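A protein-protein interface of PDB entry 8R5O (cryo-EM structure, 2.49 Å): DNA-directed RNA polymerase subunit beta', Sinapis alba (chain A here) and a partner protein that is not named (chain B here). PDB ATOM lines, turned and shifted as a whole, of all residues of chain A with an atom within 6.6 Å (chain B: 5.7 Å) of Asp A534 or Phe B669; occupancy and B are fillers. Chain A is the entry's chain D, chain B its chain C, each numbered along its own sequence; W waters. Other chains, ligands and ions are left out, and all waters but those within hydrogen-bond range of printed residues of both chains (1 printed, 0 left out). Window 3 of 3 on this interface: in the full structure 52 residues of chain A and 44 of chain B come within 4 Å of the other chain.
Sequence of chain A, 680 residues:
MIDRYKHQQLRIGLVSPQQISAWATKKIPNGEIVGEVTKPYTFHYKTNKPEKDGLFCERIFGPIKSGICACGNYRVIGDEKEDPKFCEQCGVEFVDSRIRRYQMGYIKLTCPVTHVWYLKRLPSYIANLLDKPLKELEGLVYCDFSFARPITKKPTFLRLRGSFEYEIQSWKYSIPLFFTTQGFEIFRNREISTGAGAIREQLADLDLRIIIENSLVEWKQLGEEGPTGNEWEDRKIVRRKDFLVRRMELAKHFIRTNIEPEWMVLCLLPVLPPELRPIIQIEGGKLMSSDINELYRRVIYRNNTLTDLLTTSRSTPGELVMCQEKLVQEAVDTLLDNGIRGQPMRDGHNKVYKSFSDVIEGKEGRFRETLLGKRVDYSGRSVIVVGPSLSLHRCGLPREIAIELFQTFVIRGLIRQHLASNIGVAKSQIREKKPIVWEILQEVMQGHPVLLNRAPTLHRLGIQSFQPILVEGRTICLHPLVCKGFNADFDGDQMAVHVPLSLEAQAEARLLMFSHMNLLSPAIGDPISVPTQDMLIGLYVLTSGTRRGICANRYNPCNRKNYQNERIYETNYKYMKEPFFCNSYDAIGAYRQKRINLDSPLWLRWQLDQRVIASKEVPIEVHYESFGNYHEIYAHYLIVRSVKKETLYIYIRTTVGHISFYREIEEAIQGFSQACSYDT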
ATOM      1  N   VAL A 386     -14.438 -20.554   7.523  1.00  0.00           N
ATOM      2  CA  VAL A 386     -14.377 -21.956   7.133  1.00  0.00           C
ATOM      3  C   VAL A 386     -13.783 -22.793   8.261  1.00  0.00           C
ATOM      4  O   VAL A 386     -12.832 -22.380   8.938  1.00  0.00           O
ATOM      5  CB  VAL A 386     -13.569 -22.113   5.831  1.00  0.00           C
ATOM      6  CG1 VAL A 386     -12.124 -21.661   6.026  1.00  0.00           C
ATOM      7  CG2 VAL A 386     -13.623 -23.549   5.336  1.00  0.00           C
ATOM      8  N   PRO A 480     -16.126 -26.671   4.666  1.00  0.00           N
ATOM      9  CA  PRO A 480     -15.676 -25.999   3.433  1.00  0.00           C
ATOM     10  C   PRO A 480     -16.618 -26.149   2.251  1.00  0.00           C
ATOM     11  O   PRO A 480     -16.531 -25.350   1.312  1.00  0.00           O
ATOM     12  CB  PRO A 480     -14.316 -26.654   3.153  1.00  0.00           C
ATOM     13  CG  PRO A 480     -14.373 -27.963   3.862  1.00  0.00           C
ATOM     14  CD  PRO A 480     -15.176 -27.709   5.097  1.00  0.00           C
ATOM     15  N   LEU A 481     -17.518 -27.133   2.259  1.00  0.00           N
ATOM     16  CA  LEU A 481     -18.461 -27.328   1.165  1.00  0.00           C
ATOM     17  C   LEU A 481     -19.772 -26.569   1.368  1.00  0.00           C
ATOM     18  O   LEU A 481     -20.803 -26.963   0.808  1.00  0.00           O
ATOM     19  CB  LEU A 481     -18.732 -28.821   0.969  1.00  0.00           C
ATOM     20  CG  LEU A 481     -17.488 -29.693   0.786  1.00  0.00           C
ATOM     21  CD1 LEU A 481     -17.795 -31.145   1.105  1.00  0.00           C
ATOM     22  CD2 LEU A 481     -16.937 -29.564  -0.627  1.00  0.00           C
ATOM     23  N   VAL A 482     -19.761 -25.493   2.150  1.00  0.00           N
ATOM     24  CA  VAL A 482     -20.950 -24.667   2.346  1.00  0.00           C
ATOM     25  C   VAL A 482     -20.553 -23.250   2.748  1.00  0.00           C
ATOM     26  O   VAL A 482     -19.369 -22.933   2.849  1.00  0.00           O
ATOM     27  CB  VAL A 482     -21.893 -25.273   3.400  1.00  0.00           C
ATOM     28  CG1 VAL A 482     -21.356 -25.026   4.796  1.00  0.00           C
ATOM     29  CG2 VAL A 482     -23.291 -24.696   3.254  1.00  0.00           C
ATOM     30  N   THR A 532     -13.344 -29.964  -4.364  1.00  0.00           N
ATOM     31  CA  THR A 532     -12.916 -28.935  -5.298  1.00  0.00           C
ATOM     32  C   THR A 532     -11.686 -28.214  -4.763  1.00  0.00           C
ATOM     33  O   THR A 532     -11.372 -28.272  -3.572  1.00  0.00           O
ATOM     34  CB  THR A 532     -14.028 -27.906  -5.567  1.00  0.00           C
ATOM     35  OG1 THR A 532     -14.529 -27.399  -4.325  1.00  0.00           O
ATOM     36  CG2 THR A 532     -15.166 -28.530  -6.361  1.00  0.00           C
ATOM     37  N   GLN A 533     -10.989 -27.539  -5.677  1.00  0.00           N
ATOM     38  CA  GLN A 533      -9.902 -26.603  -5.366  1.00  0.00           C
ATOM     39  C   GLN A 533      -8.806 -27.336  -4.601  1.00  0.00           C
ATOM     40  O   GLN A 533      -8.237 -28.295  -5.151  1.00  0.00           O
ATOM     41  CB  GLN A 533     -10.504 -25.385  -4.666  1.00  0.00           C
ATOM     42  CG  GLN A 533     -11.596 -24.698  -5.469  1.00  0.00           C
ATOM     43  CD  GLN A 533     -12.003 -23.364  -4.884  1.00  0.00           C
ATOM     44  OE1 GLN A 533     -11.159 -22.569  -4.471  1.00  0.00           O
ATOM     45  NE2 GLN A 533     -13.304 -23.109  -4.844  1.00  0.00           N
ATOM     46  N   ASP A 534      -8.469 -26.936  -3.372  1.00  0.00           N
ATOM     47  CA  ASP A 534      -7.333 -27.531  -2.674  1.00  0.00           C
ATOM     48  C   ASP A 534      -7.555 -29.008  -2.374  1.00  0.00           C
ATOM     49  O   ASP A 534      -6.590 -29.779  -2.331  1.00  0.00           O
ATOM     50  CB  ASP A 534      -7.051 -26.761  -1.387  1.00  0.00           C
ATOM     51  CG  ASP A 534      -6.934 -25.270  -1.618  1.00  0.00           C
ATOM     52  OD1 ASP A 534      -7.982 -24.597  -1.711  1.00  0.00           O
ATOM     53  OD2 ASP A 534      -5.793 -24.774  -1.723  1.00  0.00           O
ATOM     54  N   MET A 535      -8.804 -29.418  -2.151  1.00  0.00           N
ATOM     55  CA  MET A 535      -9.095 -30.840  -1.994  1.00  0.00           C
ATOM     56  C   MET A 535      -8.741 -31.609  -3.258  1.00  0.00           C
ATOM     57  O   MET A 535      -8.211 -32.723  -3.191  1.00  0.00           O
ATOM     58  CB  MET A 535     -10.570 -31.039  -1.650  1.00  0.00           C
ATOM     59  CG  MET A 535     -10.978 -30.515  -0.289  1.00  0.00           C
ATOM     60  SD  MET A 535     -12.768 -30.422  -0.090  1.00  0.00           S
ATOM     61  CE  MET A 535     -13.144 -28.916  -0.980  1.00  0.00           C
ATOM     62  N   LEU A 536      -9.025 -31.025  -4.421  1.00  0.00           N
ATOM     63  CA  LEU A 536      -8.847 -31.729  -5.683  1.00  0.00           C
ATOM     64  C   LEU A 536      -7.378 -31.849  -6.074  1.00  0.00           C
ATOM     65  O   LEU A 536      -6.963 -32.890  -6.593  1.00  0.00           O
ATOM     66  CB  LEU A 536      -9.644 -31.024  -6.779  1.00  0.00           C
ATOM     67  CG  LEU A 536      -9.859 -31.817  -8.064  1.00  0.00           C
ATOM     68  CD1 LEU A 536     -10.280 -33.234  -7.733  1.00  0.00           C
ATOM     69  CD2 LEU A 536     -10.910 -31.133  -8.914  1.00  0.00           C
ATOM     70  N   ILE A 537      -6.574 -30.806  -5.843  1.00  0.00           N
ATOM     71  CA  ILE A 537      -5.156 -30.895  -6.181  1.00  0.00           C
ATOM     72  C   ILE A 537      -4.460 -31.921  -5.299  1.00  0.00           C
ATOM     73  O   ILE A 537      -3.558 -32.636  -5.751  1.00  0.00           O
ATOM     74  CB  ILE A 537      -4.468 -29.521  -6.084  1.00  0.00           C
ATOM     75  CG1 ILE A 537      -4.765 -28.860  -4.743  1.00  0.00           C
ATOM     76  CG2 ILE A 537      -4.858 -28.630  -7.247  1.00  0.00           C
ATOM     77  CD1 ILE A 537      -4.093 -27.535  -4.570  1.00  0.00           C
ATOM     78  N   GLY A 538      -4.860 -32.008  -4.029  1.00  0.00           N
ATOM     79  CA  GLY A 538      -4.266 -32.995  -3.144  1.00  0.00           C
ATOM     80  C   GLY A 538      -4.455 -34.412  -3.645  1.00  0.00           C
ATOM     81  O   GLY A 538      -3.528 -35.222  -3.606  1.00  0.00           O
ATOM     82  N   LEU A 539      -5.657 -34.730  -4.127  1.00  0.00           N
ATOM     83  CA  LEU A 539      -5.890 -36.043  -4.721  1.00  0.00           C
ATOM     84  C   LEU A 539      -5.116 -36.205  -6.023  1.00  0.00           C
ATOM     85  O   LEU A 539      -4.592 -37.286  -6.308  1.00  0.00           O
ATOM     86  CB  LEU A 539      -7.384 -36.258  -4.958  1.00  0.00           C
ATOM     87  CG  LEU A 539      -8.298 -36.081  -3.745  1.00  0.00           C
ATOM     88  CD1 LEU A 539      -9.748 -36.331  -4.125  1.00  0.00           C
ATOM     89  CD2 LEU A 539      -7.867 -36.995  -2.610  1.00  0.00           C
ATOM     90  N   PRO B 663      -1.335 -23.946   0.111  1.00  0.00           N
ATOM     91  CA  PRO B 663      -2.491 -24.431   0.873  1.00  0.00           C
ATOM     92  C   PRO B 663      -2.044 -24.995   2.213  1.00  0.00           C
ATOM     93  O   PRO B 663      -1.004 -25.646   2.313  1.00  0.00           O
ATOM     94  CB  PRO B 663      -3.080 -25.519  -0.029  1.00  0.00           C
ATOM     95  CG  PRO B 663      -1.938 -25.976  -0.857  1.00  0.00           C
ATOM     96  CD  PRO B 663      -1.052 -24.784  -1.065  1.00  0.00           C
ATOM     97  N   GLY B 666      -6.651 -26.582   4.486  1.00  0.00           N
ATOM     98  CA  GLY B 666      -7.978 -26.048   4.273  1.00  0.00           C
ATOM     99  C   GLY B 666      -8.313 -24.802   5.060  1.00  0.00           C
ATOM    100  O   GLY B 666      -9.417 -24.269   4.896  1.00  0.00           O
ATOM    101  N   TYR B 667      -7.406 -24.314   5.907  1.00  0.00           N
ATOM    102  CA  TYR B 667      -7.660 -23.088   6.651  1.00  0.00           C
ATOM    103  C   TYR B 667      -7.503 -21.835   5.801  1.00  0.00           C
ATOM    104  O   TYR B 667      -7.906 -20.756   6.243  1.00  0.00           O
ATOM    105  CB  TYR B 667      -6.743 -23.005   7.872  1.00  0.00           C
ATOM    106  CG  TYR B 667      -7.089 -24.018   8.935  1.00  0.00           C
ATOM    107  CD1 TYR B 667      -8.112 -23.779   9.843  1.00  0.00           C
ATOM    108  CD2 TYR B 667      -6.407 -25.221   9.019  1.00  0.00           C
ATOM    109  CE1 TYR B 667      -8.439 -24.708  10.809  1.00  0.00           C
ATOM    110  CE2 TYR B 667      -6.724 -26.153   9.981  1.00  0.00           C
ATOM    111  CZ  TYR B 667      -7.740 -25.894  10.874  1.00  0.00           C
ATOM    112  OH  TYR B 667      -8.054 -26.829  11.832  1.00  0.00           O
ATOM    113  N   ASN B 668      -6.931 -21.947   4.603  1.00  0.00           N
ATOM    114  CA  ASN B 668      -6.925 -20.850   3.644  1.00  0.00           C
ATOM    115  C   ASN B 668      -7.727 -21.210   2.398  1.00  0.00           C
ATOM    116  O   ASN B 668      -7.450 -20.715   1.307  1.00  0.00           O
ATOM    117  CB  ASN B 668      -5.498 -20.433   3.280  1.00  0.00           C
ATOM    118  CG  ASN B 668      -4.637 -21.593   2.827  1.00  0.00           C
ATOM    119  OD1 ASN B 668      -5.117 -22.712   2.647  1.00  0.00           O
ATOM    120  ND2 ASN B 668      -3.353 -21.328   2.634  1.00  0.00           N
ATOM    121  N   PHE B 669      -8.723 -22.077   2.559  1.00  0.00           N
ATOM    122  CA  PHE B 669      -9.604 -22.444   1.458  1.00  0.00           C
ATOM    123  C   PHE B 669     -10.300 -21.208   0.901  1.00  0.00           C
ATOM    124  O   PHE B 669     -10.879 -20.417   1.651  1.00  0.00           O
ATOM    125  CB  PHE B 669     -10.629 -23.468   1.946  1.00  0.00           C
ATOM    126  CG  PHE B 669     -11.549 -23.980   0.875  1.00  0.00           C
ATOM    127  CD1 PHE B 669     -11.117 -24.931  -0.034  1.00  0.00           C
ATOM    128  CD2 PHE B 669     -12.857 -23.534   0.798  1.00  0.00           C
ATOM    129  CE1 PHE B 669     -11.968 -25.412  -1.012  1.00  0.00           C
ATOM    130  CE2 PHE B 669     -13.710 -24.010  -0.177  1.00  0.00           C
ATOM    131  CZ  PHE B 669     -13.265 -24.950  -1.084  1.00  0.00           C
ATOM    132  N   GLU B 670     -10.236 -21.047  -0.422  1.00  0.00           N
ATOM    133  CA  GLU B 670     -10.782 -19.887  -1.135  1.00  0.00           C
ATOM    134  C   GLU B 670     -10.068 -18.640  -0.624  1.00  0.00           C
ATOM    135  O   GLU B 670      -8.834 -18.566  -0.746  1.00  0.00           O
ATOM    136  CB  GLU B 670     -12.307 -19.879  -1.010  1.00  0.00           C
ATOM    137  CG  GLU B 670     -12.995 -20.995  -1.765  1.00  0.00           C
ATOM    138  CD  GLU B 670     -14.502 -20.951  -1.615  1.00  0.00           C
ATOM    139  OE1 GLU B 670     -15.015 -19.951  -1.073  1.00  0.00           O
ATOM    140  OE2 GLU B 670     -15.174 -21.916  -2.035  1.00  0.00           O
ATOM    141  N   ASP B 671     -10.768 -17.654  -0.066  1.00  0.00           N
ATOM    142  CA  ASP B 671     -10.156 -16.411   0.380  1.00  0.00           C
ATOM    143  C   ASP B 671      -9.806 -16.414   1.861  1.00  0.00           C
ATOM    144  O   ASP B 671      -9.407 -15.376   2.390  1.00  0.00           O
ATOM    145  CB  ASP B 671     -11.071 -15.227   0.063  1.00  0.00           C
ATOM    146  CG  ASP B 671     -11.078 -14.873  -1.412  1.00  0.00           C
ATOM    147  OD1 ASP B 671     -10.294 -15.479  -2.174  1.00  0.00           O
ATOM    148  OD2 ASP B 671     -11.866 -13.993  -1.811  1.00  0.00           O
ATOM    149  N   ALA B 672      -9.947 -17.546   2.543  1.00  0.00           N
ATOM    150  CA  ALA B 672      -9.553 -17.611   3.942  1.00  0.00           C
ATOM    151  C   ALA B 672      -8.047 -17.408   4.074  1.00  0.00           C
ATOM    152  O   ALA B 672      -7.273 -17.739   3.173  1.00  0.00           O
ATOM    153  CB  ALA B 672      -9.971 -18.947   4.553  1.00  0.00           C
ATOM    154  N   ASN B 855      -3.684 -18.603   0.042  1.00  0.00           N
ATOM    155  CA  ASN B 855      -3.980 -19.670  -0.904  1.00  0.00           C
ATOM    156  C   ASN B 855      -3.423 -19.314  -2.277  1.00  0.00           C
ATOM    157  O   ASN B 855      -3.760 -18.252  -2.813  1.00  0.00           O
ATOM    158  CB  ASN B 855      -5.486 -19.893  -0.979  1.00  0.00           C
ATOM    159  CG  ASN B 855      -5.862 -21.074  -1.848  1.00  0.00           C
ATOM    160  OD1 ASN B 855      -5.119 -22.048  -1.953  1.00  0.00           O
ATOM    161  ND2 ASN B 855      -7.026 -20.993  -2.480  1.00  0.00           N
ATOM    162  N   PRO B 856      -2.576 -20.155  -2.879  1.00  0.00           N
ATOM    163  CA  PRO B 856      -2.051 -19.831  -4.215  1.00  0.00           C
ATOM    164  C   PRO B 856      -3.062 -20.012  -5.333  1.00  0.00           C
ATOM    165  O   PRO B 856      -2.839 -19.486  -6.431  1.00  0.00           O
ATOM    166  CB  PRO B 856      -0.879 -20.807  -4.372  1.00  0.00           C
ATOM    167  CG  PRO B 856      -1.273 -21.975  -3.547  1.00  0.00           C
ATOM    168  CD  PRO B 856      -2.045 -21.429  -2.373  1.00  0.00           C
ATOM    169  N   LEU B 857      -4.156 -20.738  -5.098  1.00  0.00           N
ATOM    170  CA  LEU B 857      -5.164 -20.948  -6.128  1.00  0.00           C
ATOM    171  C   LEU B 857      -5.979 -19.695  -6.418  1.00  0.00           C
ATOM    172  O   LEU B 857      -6.708 -19.669  -7.414  1.00  0.00           O
ATOM    173  CB  LEU B 857      -6.103 -22.091  -5.729  1.00  0.00           C
ATOM    174  CG  LEU B 857      -5.629 -23.528  -5.977  1.00  0.00           C
ATOM    175  CD1 LEU B 857      -4.473 -23.915  -5.064  1.00  0.00           C
ATOM    176  CD2 LEU B 857      -6.782 -24.508  -5.823  1.00  0.00           C
HETATM  177  O   HOH W   1      -6.206 -24.856   1.595  1.00  0.00           O
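ND2 of Asn B855 lies within hydrogen-bond range of O of Glu B670 (3.5 Å).
Among the printed residues, pairs that only touch across the chains: Val A386 with Gly B666, Val A386 with Ala B672, Pro A480 with Phe B669, Thr A532 with Phe B669, Gln A533 with Phe B669, Gln A533 with Glu B670, Gln A533 with Leu B857, Asp A534 with Pro B663, Asp A534 with Phe B669, Asp A534 with Leu B857, Met A535 with Phe B669 and Ile A537 with Leu B857.
Asp A534 touches just these residues of chain B: Pro B663 (3.3 Å), Phe B669 (3.6 Å), Asn B855 (2.8 Å) and Leu B857 (3.7 Å). Printed residues of chain B within 4 Å of Met A535: Phe B669 (3.7 Å). Printed residues of chain A within 4 Å of Gly B666: Val A386 (3.9 Å). The nearest residue of chain A that does not touch Phe B669 is Val A386 (4.5 Å).
Of the 11 printed residues of chain B, 7 touch a printed residue of chain A. Hydrophobic or aromatic side chains of chain B within 4 Å of the printed part of chain A: Pro B663, Phe B669, Ala B672 and Leu B857. Along chain B the printed residues that touch a printed residue of chain A span positions 663 to 857. Of the 12 printed residues of chain A, 7 touch a printed residue of chain B. Among the printed residues, no Asp or Glu carboxylate lies within 4 Å of a Lys or Arg side-chain nitrogen of the other chain.
Water W1 lies within hydrogen-bond range of the side-chain amide oxygen of Asn B668, the side-chain carboxylate of Asp A534 and the backbone NH of Gly B666.
OD2 of Asp A534 sits close to OD1 of Asn B855, 2.8 Å away.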
